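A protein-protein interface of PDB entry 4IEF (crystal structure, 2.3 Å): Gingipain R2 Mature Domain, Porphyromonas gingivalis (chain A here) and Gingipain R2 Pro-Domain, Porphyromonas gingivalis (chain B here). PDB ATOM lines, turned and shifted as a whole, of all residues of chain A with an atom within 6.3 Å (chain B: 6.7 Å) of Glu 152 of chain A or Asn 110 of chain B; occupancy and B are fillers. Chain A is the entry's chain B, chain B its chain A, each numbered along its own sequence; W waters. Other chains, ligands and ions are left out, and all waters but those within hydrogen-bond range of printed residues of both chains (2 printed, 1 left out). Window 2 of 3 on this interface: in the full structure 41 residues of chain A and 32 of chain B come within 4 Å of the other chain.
Of the 11 printed residues of chain B, 7 touch a printed residue of chain A.
Printed residues of chain B that touch a printed residue of chain A: Ile 105, Ser 106, Arg 107, Glu 109, Asn 110, Pro 111 and Asp 112.
Hydrophobic or aromatic side chains of chain B within 4 Å of the printed part of chain A: Pro 111.
Hydrophobic or aromatic side chains of chain A that line the printed part of chain B: His 211 and Trp 284.
Among the printed residues, 13 pairs touch across the chains.
Among the printed residues, Asp or Glu carboxylates within 4 Å of a Lys or Arg side-chain nitrogen of the other chain: Asp 163 of chain A with Arg 107 of chain B (2.8 Å).
Glu 152 of chain A touches just these residues of chain B: Glu 109, Asn 110, Pro 111 and Asp 112.
Of chain A, only Glu 152 (3.3 Å) comes within 4 Å of Asn 110 of chain B.
Of the printed residues of chain A, Asp 112 of chain B touches Glu 152 (3.6 Å) and Gly 153 (3.3 Å).
Of the printed residues of chain B, His 211 of chain A touches Arg 107 (2.3 Å) and Glu 109 (3.2 Å).
Of the printed residues of chain A, Ser 106 of chain B touches Trp 284 (3.96 Å).
The nearest residue of chain A that does not touch Asn 110 of chain B is His 211 of chain A (4.8 Å).
Water W1 lies within hydrogen-bond range of the backbone carbonyl oxygen (O) of Ala 151 of chain A and the side-chain carboxylate (OD2) of Asp 112 of chain B.
Water W2 bridges the backbone NH (N) of Ile 105 of chain B (3.0 Å) and the backbone NH (N) of Trp 284 of chain A (3.4 Å).
The side-chain amino group of Lys 102 of chain B sits at hydrogen-bond distance from the backbone carbonyl oxygen of Pro 111 of chain B, 2.8 Å away.
OE1 of Glu 109 of chain B is in hydrogen-bond range of N of Ser 106 of chain B (3.4 Å).
The backbone NH of Asp 112 of chain B sits close to the side-chain amide oxygen of Asn 110 of chain B.
ND2 of Asn 110 of chain B is in hydrogen-bond range of OE1 of Gln 113 of chain B, 3.2 Å away.
OG of Ser 150 of chain A sits close to N of Glu 152 of chain A (3.4 Å).
The backbone NH (N) of Asp 163 of chain A sits at hydrogen-bond distance from the backbone carbonyl oxygen (O) of Glu 152 of chain A.
The backbone carbonyl oxygen (O) of Ile 105 of chain B sits at hydrogen-bond distance from the backbone NH (N) of Trp 284 of chain A.
OD2 of Asp 163 of chain A lies within salt-bridge range of NH1 of Arg 107 of chain B (2.8 Å).
The guanidinium group of Arg 107 of chain B lies within hydrogen-bond range of the backbone carbonyl oxygen of Trp 284 of chain A (3.1 Å).
The side-chain amide oxygen of Asn 110 of chain B sits close to the side-chain carboxylate of Glu 152 of chain A (3.3 Å).
OD1 of Asp 112 of chain B lies within hydrogen-bond range of N of Gly 153 of chain A (3.3 Å).
A ring nitrogen (ND1) of His 211 of chain A sits close to the backbone carbonyl oxygen of Arg 107 of chain B (2.3 Å).
OE1 of Glu 152 of chain A touches O of Glu 109 of chain B, 3.9 Å away.
Glu 152 of chain A touches Pro 111 of chain B.
Asp 112 of chain B touches Glu 152 of chain A (OD2 to CA, 3.6 Å).
CE1 of His 211 of chain A touches O of Glu 109 of chain B, at 3.2 Å.
Ser 106 of chain B touches Trp 284 of chain A (O to CE3, 3.96 Å).
Trp 284 of chain A touches Glu 109 of chain B (CZ3 to O, 3.4 Å).
Trp 284 of chain A touches Pro 111 of chain B.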
ATOM      1  N   ALA A 149      16.928  21.833  38.656  1.00  0.00           N
ATOM      2  CA  ALA A 149      16.936  21.996  37.202  1.00  0.00           C
ATOM      3  C   ALA A 149      18.290  22.374  36.642  1.00  0.00           C
ATOM      4  O   ALA A 149      19.040  23.127  37.272  1.00  0.00           O
ATOM      5  CB  ALA A 149      15.926  23.049  36.790  1.00  0.00           C
ATOM      6  N   SER A 150      18.566  21.898  35.407  1.00  0.00           N
ATOM      7  CA  SER A 150      19.767  22.245  34.648  1.00  0.00           C
ATOM      8  C   SER A 150      19.583  23.640  34.039  1.00  0.00           C
ATOM      9  O   SER A 150      18.462  24.149  34.004  1.00  0.00           O
ATOM     10  CB  SER A 150      20.051  21.198  33.566  1.00  0.00           C
ATOM     11  OG  SER A 150      19.182  21.299  32.451  1.00  0.00           O
ATOM     12  N   ALA A 151      20.671  24.242  33.548  1.00  0.00           N
ATOM     13  CA  ALA A 151      20.649  25.557  32.902  1.00  0.00           C
ATOM     14  C   ALA A 151      20.407  25.424  31.375  1.00  0.00           C
ATOM     15  O   ALA A 151      20.640  26.371  30.618  1.00  0.00           O
ATOM     16  CB  ALA A 151      21.955  26.288  33.180  1.00  0.00           C
ATOM     17  N   GLU A 152      19.896  24.260  30.937  1.00  0.00           N
ATOM     18  CA  GLU A 152      19.633  23.963  29.526  1.00  0.00           C
ATOM     19  C   GLU A 152      18.128  23.869  29.224  1.00  0.00           C
ATOM     20  O   GLU A 152      17.304  23.929  30.139  1.00  0.00           O
ATOM     21  CB  GLU A 152      20.340  22.664  29.121  1.00  0.00           C
ATOM     22  CG  GLU A 152      21.857  22.720  29.263  1.00  0.00           C
ATOM     23  CD  GLU A 152      22.590  21.409  29.058  1.00  0.00           C
ATOM     24  OE1 GLU A 152      21.992  20.470  28.486  1.00  0.00           O
ATOM     25  OE2 GLU A 152      23.779  21.329  29.435  1.00  0.00           O
ATOM     26  N   GLY A 153      17.803  23.748  27.938  1.00  0.00           N
ATOM     27  CA  GLY A 153      16.435  23.632  27.452  1.00  0.00           C
ATOM     28  C   GLY A 153      15.945  24.891  26.783  1.00  0.00           C
ATOM     29  O   GLY A 153      16.347  25.998  27.157  1.00  0.00           O
ATOM     30  N   GLY A 154      15.081  24.725  25.791  1.00  0.00           N
ATOM     31  CA  GLY A 154      14.531  25.840  25.033  1.00  0.00           C
ATOM     32  C   GLY A 154      13.305  25.496  24.210  1.00  0.00           C
ATOM     33  O   GLY A 154      12.476  24.696  24.653  1.00  0.00           O
ATOM     34  N   GLU A 161       9.778  24.939  27.016  1.00  0.00           N
ATOM     35  CA  GLU A 161      10.314  25.370  28.297  1.00  0.00           C
ATOM     36  C   GLU A 161      11.680  24.833  28.571  1.00  0.00           C
ATOM     37  O   GLU A 161      11.956  23.660  28.308  1.00  0.00           O
ATOM     38  CB  GLU A 161       9.404  24.929  29.450  1.00  0.00           C
ATOM     39  CG  GLU A 161       7.980  25.449  29.421  1.00  0.00           C
ATOM     40  CD  GLU A 161       7.082  24.641  30.329  1.00  0.00           C
ATOM     41  OE1 GLU A 161       7.635  23.825  31.091  1.00  0.00           O
ATOM     42  OE2 GLU A 161       5.844  24.815  30.294  1.00  0.00           O
ATOM     43  N   SER A 162      12.511  25.684  29.189  1.00  0.00           N
ATOM     44  CA  SER A 162      13.821  25.320  29.696  1.00  0.00           C
ATOM     45  C   SER A 162      13.580  24.495  30.949  1.00  0.00           C
ATOM     46  O   SER A 162      12.496  24.616  31.536  1.00  0.00           O
ATOM     47  CB  SER A 162      14.620  26.579  30.013  1.00  0.00           C
ATOM     48  OG  SER A 162      14.134  27.177  31.204  1.00  0.00           O
ATOM     49  N   ASP A 163      14.570  23.701  31.397  1.00  0.00           N
ATOM     50  CA  ASP A 163      14.426  22.888  32.610  1.00  0.00           C
ATOM     51  C   ASP A 163      14.060  23.746  33.843  1.00  0.00           C
ATOM     52  O   ASP A 163      13.261  23.300  34.667  1.00  0.00           O
ATOM     53  CB  ASP A 163      15.688  22.042  32.865  1.00  0.00           C
ATOM     54  CG  ASP A 163      15.824  20.860  31.913  1.00  0.00           C
ATOM     55  OD1 ASP A 163      14.935  20.682  31.048  1.00  0.00           O
ATOM     56  OD2 ASP A 163      16.822  20.119  32.025  1.00  0.00           O
ATOM     57  N   ILE A 164      14.578  24.985  33.915  1.00  0.00           N
ATOM     58  CA  ILE A 164      14.302  25.968  34.969  1.00  0.00           C
ATOM     59  C   ILE A 164      12.841  26.453  34.850  1.00  0.00           C
ATOM     60  O   ILE A 164      12.131  26.436  35.858  1.00  0.00           O
ATOM     61  CB  ILE A 164      15.342  27.129  34.929  1.00  0.00           C
ATOM     62  CG1 ILE A 164      16.679  26.660  35.555  1.00  0.00           C
ATOM     63  CG2 ILE A 164      14.818  28.418  35.602  1.00  0.00           C
ATOM     64  CD1 ILE A 164      17.973  27.502  35.169  1.00  0.00           C
ATOM     65  N   HIS A 211      20.500  16.377  33.558  1.00  0.00           N
ATOM     66  CA  HIS A 211      21.347  15.268  33.140  1.00  0.00           C
ATOM     67  C   HIS A 211      21.616  14.346  34.300  1.00  0.00           C
ATOM     68  O   HIS A 211      21.554  14.751  35.460  1.00  0.00           O
ATOM     69  CB  HIS A 211      22.675  15.783  32.564  1.00  0.00           C
ATOM     70  CG  HIS A 211      22.507  16.704  31.397  1.00  0.00           C
ATOM     71  ND1 HIS A 211      22.453  16.225  30.105  1.00  0.00           N
ATOM     72  CD2 HIS A 211      22.389  18.049  31.369  1.00  0.00           C
ATOM     73  CE1 HIS A 211      22.309  17.287  29.332  1.00  0.00           C
ATOM     74  NE2 HIS A 211      22.259  18.404  30.048  1.00  0.00           N
ATOM     75  N   TRP A 284      14.667  14.397  25.704  1.00  0.00           N
ATOM     76  CA  TRP A 284      14.551  15.712  26.318  1.00  0.00           C
ATOM     77  C   TRP A 284      13.115  16.078  26.713  1.00  0.00           C
ATOM     78  O   TRP A 284      12.873  16.408  27.874  1.00  0.00           O
ATOM     79  CB  TRP A 284      15.131  16.819  25.408  1.00  0.00           C
ATOM     80  CG  TRP A 284      15.490  18.045  26.193  1.00  0.00           C
ATOM     81  CD1 TRP A 284      14.645  19.039  26.584  1.00  0.00           C
ATOM     82  CD2 TRP A 284      16.737  18.298  26.854  1.00  0.00           C
ATOM     83  NE1 TRP A 284      15.299  19.927  27.402  1.00  0.00           N
ATOM     84  CE2 TRP A 284      16.584  19.493  27.592  1.00  0.00           C
ATOM     85  CE3 TRP A 284      17.976  17.636  26.884  1.00  0.00           C
ATOM     86  CZ2 TRP A 284      17.620  20.043  28.348  1.00  0.00           C
ATOM     87  CZ3 TRP A 284      18.989  18.160  27.666  1.00  0.00           C
ATOM     88  CH2 TRP A 284      18.805  19.353  28.387  1.00  0.00           C
ATOM     89  N   LYS B 102      14.750  19.274  15.241  1.00  0.00           N
ATOM     90  CA  LYS B 102      15.997  18.713  15.758  1.00  0.00           C
ATOM     91  C   LYS B 102      15.803  17.215  16.039  1.00  0.00           C
ATOM     92  O   LYS B 102      16.770  16.502  16.318  1.00  0.00           O
ATOM     93  CB  LYS B 102      16.427  19.444  17.043  1.00  0.00           C
ATOM     94  CG  LYS B 102      16.929  20.858  16.822  1.00  0.00           C
ATOM     95  CD  LYS B 102      17.448  21.443  18.125  1.00  0.00           C
ATOM     96  CE  LYS B 102      17.794  22.900  17.964  1.00  0.00           C
ATOM     97  NZ  LYS B 102      18.404  23.465  19.196  1.00  0.00           N
ATOM     98  N   ILE B 105      15.823  14.475  20.931  1.00  0.00           N
ATOM     99  CA  ILE B 105      17.090  14.849  21.555  1.00  0.00           C
ATOM    100  C   ILE B 105      17.254  14.012  22.832  1.00  0.00           C
ATOM    101  O   ILE B 105      16.314  13.901  23.613  1.00  0.00           O
ATOM    102  CB  ILE B 105      17.164  16.385  21.838  1.00  0.00           C
ATOM    103  CG1 ILE B 105      17.086  17.201  20.531  1.00  0.00           C
ATOM    104  CG2 ILE B 105      18.430  16.753  22.638  1.00  0.00           C
ATOM    105  CD1 ILE B 105      16.750  18.698  20.717  1.00  0.00           C
ATOM    106  N   SER B 106      18.440  13.435  23.034  1.00  0.00           N
ATOM    107  CA  SER B 106      18.756  12.679  24.240  1.00  0.00           C
ATOM    108  C   SER B 106      19.227  13.641  25.327  1.00  0.00           C
ATOM    109  O   SER B 106      19.819  14.674  25.004  1.00  0.00           O
ATOM    110  CB  SER B 106      19.831  11.638  23.941  1.00  0.00           C
ATOM    111  OG  SER B 106      20.273  10.973  25.111  1.00  0.00           O
ATOM    112  N   ARG B 107      19.009  13.300  26.611  1.00  0.00           N
ATOM    113  CA  ARG B 107      19.490  14.142  27.714  1.00  0.00           C
ATOM    114  C   ARG B 107      20.999  13.898  27.939  1.00  0.00           C
ATOM    115  O   ARG B 107      21.572  14.437  28.874  1.00  0.00           O
ATOM    116  CB  ARG B 107      18.657  13.980  29.002  1.00  0.00           C
ATOM    117  CG  ARG B 107      17.322  14.687  28.863  1.00  0.00           C
ATOM    118  CD  ARG B 107      16.514  14.846  30.133  1.00  0.00           C
ATOM    119  NE  ARG B 107      15.453  15.825  29.890  1.00  0.00           N
ATOM    120  CZ  ARG B 107      15.471  17.083  30.315  1.00  0.00           C
ATOM    121  NH1 ARG B 107      16.453  17.513  31.096  1.00  0.00           N
ATOM    122  NH2 ARG B 107      14.483  17.906  30.003  1.00  0.00           N
ATOM    123  N   ALA B 108      21.645  13.137  27.039  1.00  0.00           N
ATOM    124  CA  ALA B 108      23.094  12.924  26.998  1.00  0.00           C
ATOM    125  C   ALA B 108      23.748  14.083  26.209  1.00  0.00           C
ATOM    126  O   ALA B 108      24.972  14.254  26.238  1.00  0.00           O
ATOM    127  CB  ALA B 108      23.408  11.586  26.338  1.00  0.00           C
ATOM    128  N   GLU B 109      22.905  14.879  25.517  1.00  0.00           N
ATOM    129  CA  GLU B 109      23.290  16.025  24.684  1.00  0.00           C
ATOM    130  C   GLU B 109      22.802  17.349  25.274  1.00  0.00           C
ATOM    131  O   GLU B 109      21.931  17.359  26.143  1.00  0.00           O
ATOM    132  CB  GLU B 109      22.690  15.877  23.269  1.00  0.00           C
ATOM    133  CG  GLU B 109      22.913  14.540  22.587  1.00  0.00           C
ATOM    134  CD  GLU B 109      22.318  14.495  21.192  1.00  0.00           C
ATOM    135  OE1 GLU B 109      21.145  14.078  21.049  1.00  0.00           O
ATOM    136  OE2 GLU B 109      23.013  14.929  20.245  1.00  0.00           O
ATOM    137  N   ASN B 110      23.338  18.466  24.768  1.00  0.00           N
ATOM    138  CA  ASN B 110      22.908  19.816  25.133  1.00  0.00           C
ATOM    139  C   ASN B 110      22.127  20.376  23.925  1.00  0.00           C
ATOM    140  O   ASN B 110      22.736  20.573  22.868  1.00  0.00           O
ATOM    141  CB  ASN B 110      24.107  20.707  25.529  1.00  0.00           C
ATOM    142  CG  ASN B 110      23.749  22.102  26.022  1.00  0.00           C
ATOM    143  OD1 ASN B 110      22.588  22.533  26.008  1.00  0.00           O
ATOM    144  ND2 ASN B 110      24.750  22.848  26.475  1.00  0.00           N
ATOM    145  N   PRO B 111      20.787  20.583  24.023  1.00  0.00           N
ATOM    146  CA  PRO B 111      20.021  21.056  22.850  1.00  0.00           C
ATOM    147  C   PRO B 111      20.389  22.464  22.397  1.00  0.00           C
ATOM    148  O   PRO B 111      20.212  22.786  21.220  1.00  0.00           O
ATOM    149  CB  PRO B 111      18.566  20.995  23.322  1.00  0.00           C
ATOM    150  CG  PRO B 111      18.636  21.061  24.792  1.00  0.00           C
ATOM    151  CD  PRO B 111      19.903  20.371  25.185  1.00  0.00           C
ATOM    152  N   ASP B 112      20.910  23.296  23.323  1.00  0.00           N
ATOM    153  CA  ASP B 112      21.351  24.670  23.056  1.00  0.00           C
ATOM    154  C   ASP B 112      22.571  24.667  22.120  1.00  0.00           C
ATOM    155  O   ASP B 112      22.800  25.645  21.413  1.00  0.00           O
ATOM    156  CB  ASP B 112      21.693  25.407  24.376  1.00  0.00           C
ATOM    157  CG  ASP B 112      20.763  25.177  25.572  1.00  0.00           C
ATOM    158  OD1 ASP B 112      19.645  24.645  25.371  1.00  0.00           O
ATOM    159  OD2 ASP B 112      21.151  25.543  26.704  1.00  0.00           O
ATOM    160  N   GLN B 113      23.329  23.556  22.113  1.00  0.00           N
ATOM    161  CA  GLN B 113      24.524  23.341  21.289  1.00  0.00           C
ATOM    162  C   GLN B 113      24.205  22.595  19.976  1.00  0.00           C
ATOM    163  O   GLN B 113      25.080  22.500  19.113  1.00  0.00           O
ATOM    164  CB  GLN B 113      25.578  22.564  22.085  1.00  0.00           C
ATOM    165  CG  GLN B 113      26.420  23.424  23.021  1.00  0.00           C
ATOM    166  CD  GLN B 113      27.290  22.603  23.943  1.00  0.00           C
ATOM    167  OE1 GLN B 113      27.617  23.040  25.042  1.00  0.00           O
ATOM    168  NE2 GLN B 113      27.689  21.397  23.537  1.00  0.00           N
ATOM    169  N   ILE B 114      22.967  22.075  19.822  1.00  0.00           N
ATOM    170  CA  ILE B 114      22.528  21.369  18.613  1.00  0.00           C
ATOM    171  C   ILE B 114      21.932  22.417  17.657  1.00  0.00           C
ATOM    172  O   ILE B 114      21.031  23.157  18.057  1.00  0.00           O
ATOM    173  CB  ILE B 114      21.546  20.196  18.914  1.00  0.00           C
ATOM    174  CG1 ILE B 114      22.207  19.135  19.822  1.00  0.00           C
ATOM    175  CG2 ILE B 114      21.034  19.549  17.614  1.00  0.00           C
ATOM    176  CD1 ILE B 114      21.234  18.205  20.553  1.00  0.00           C
HETATM  177  O   HOH W   1      22.024  27.463  28.506  1.00  0.00           O
HETATM  178  O   HOH W   2      13.389  15.114  22.597  1.00  0.00           O
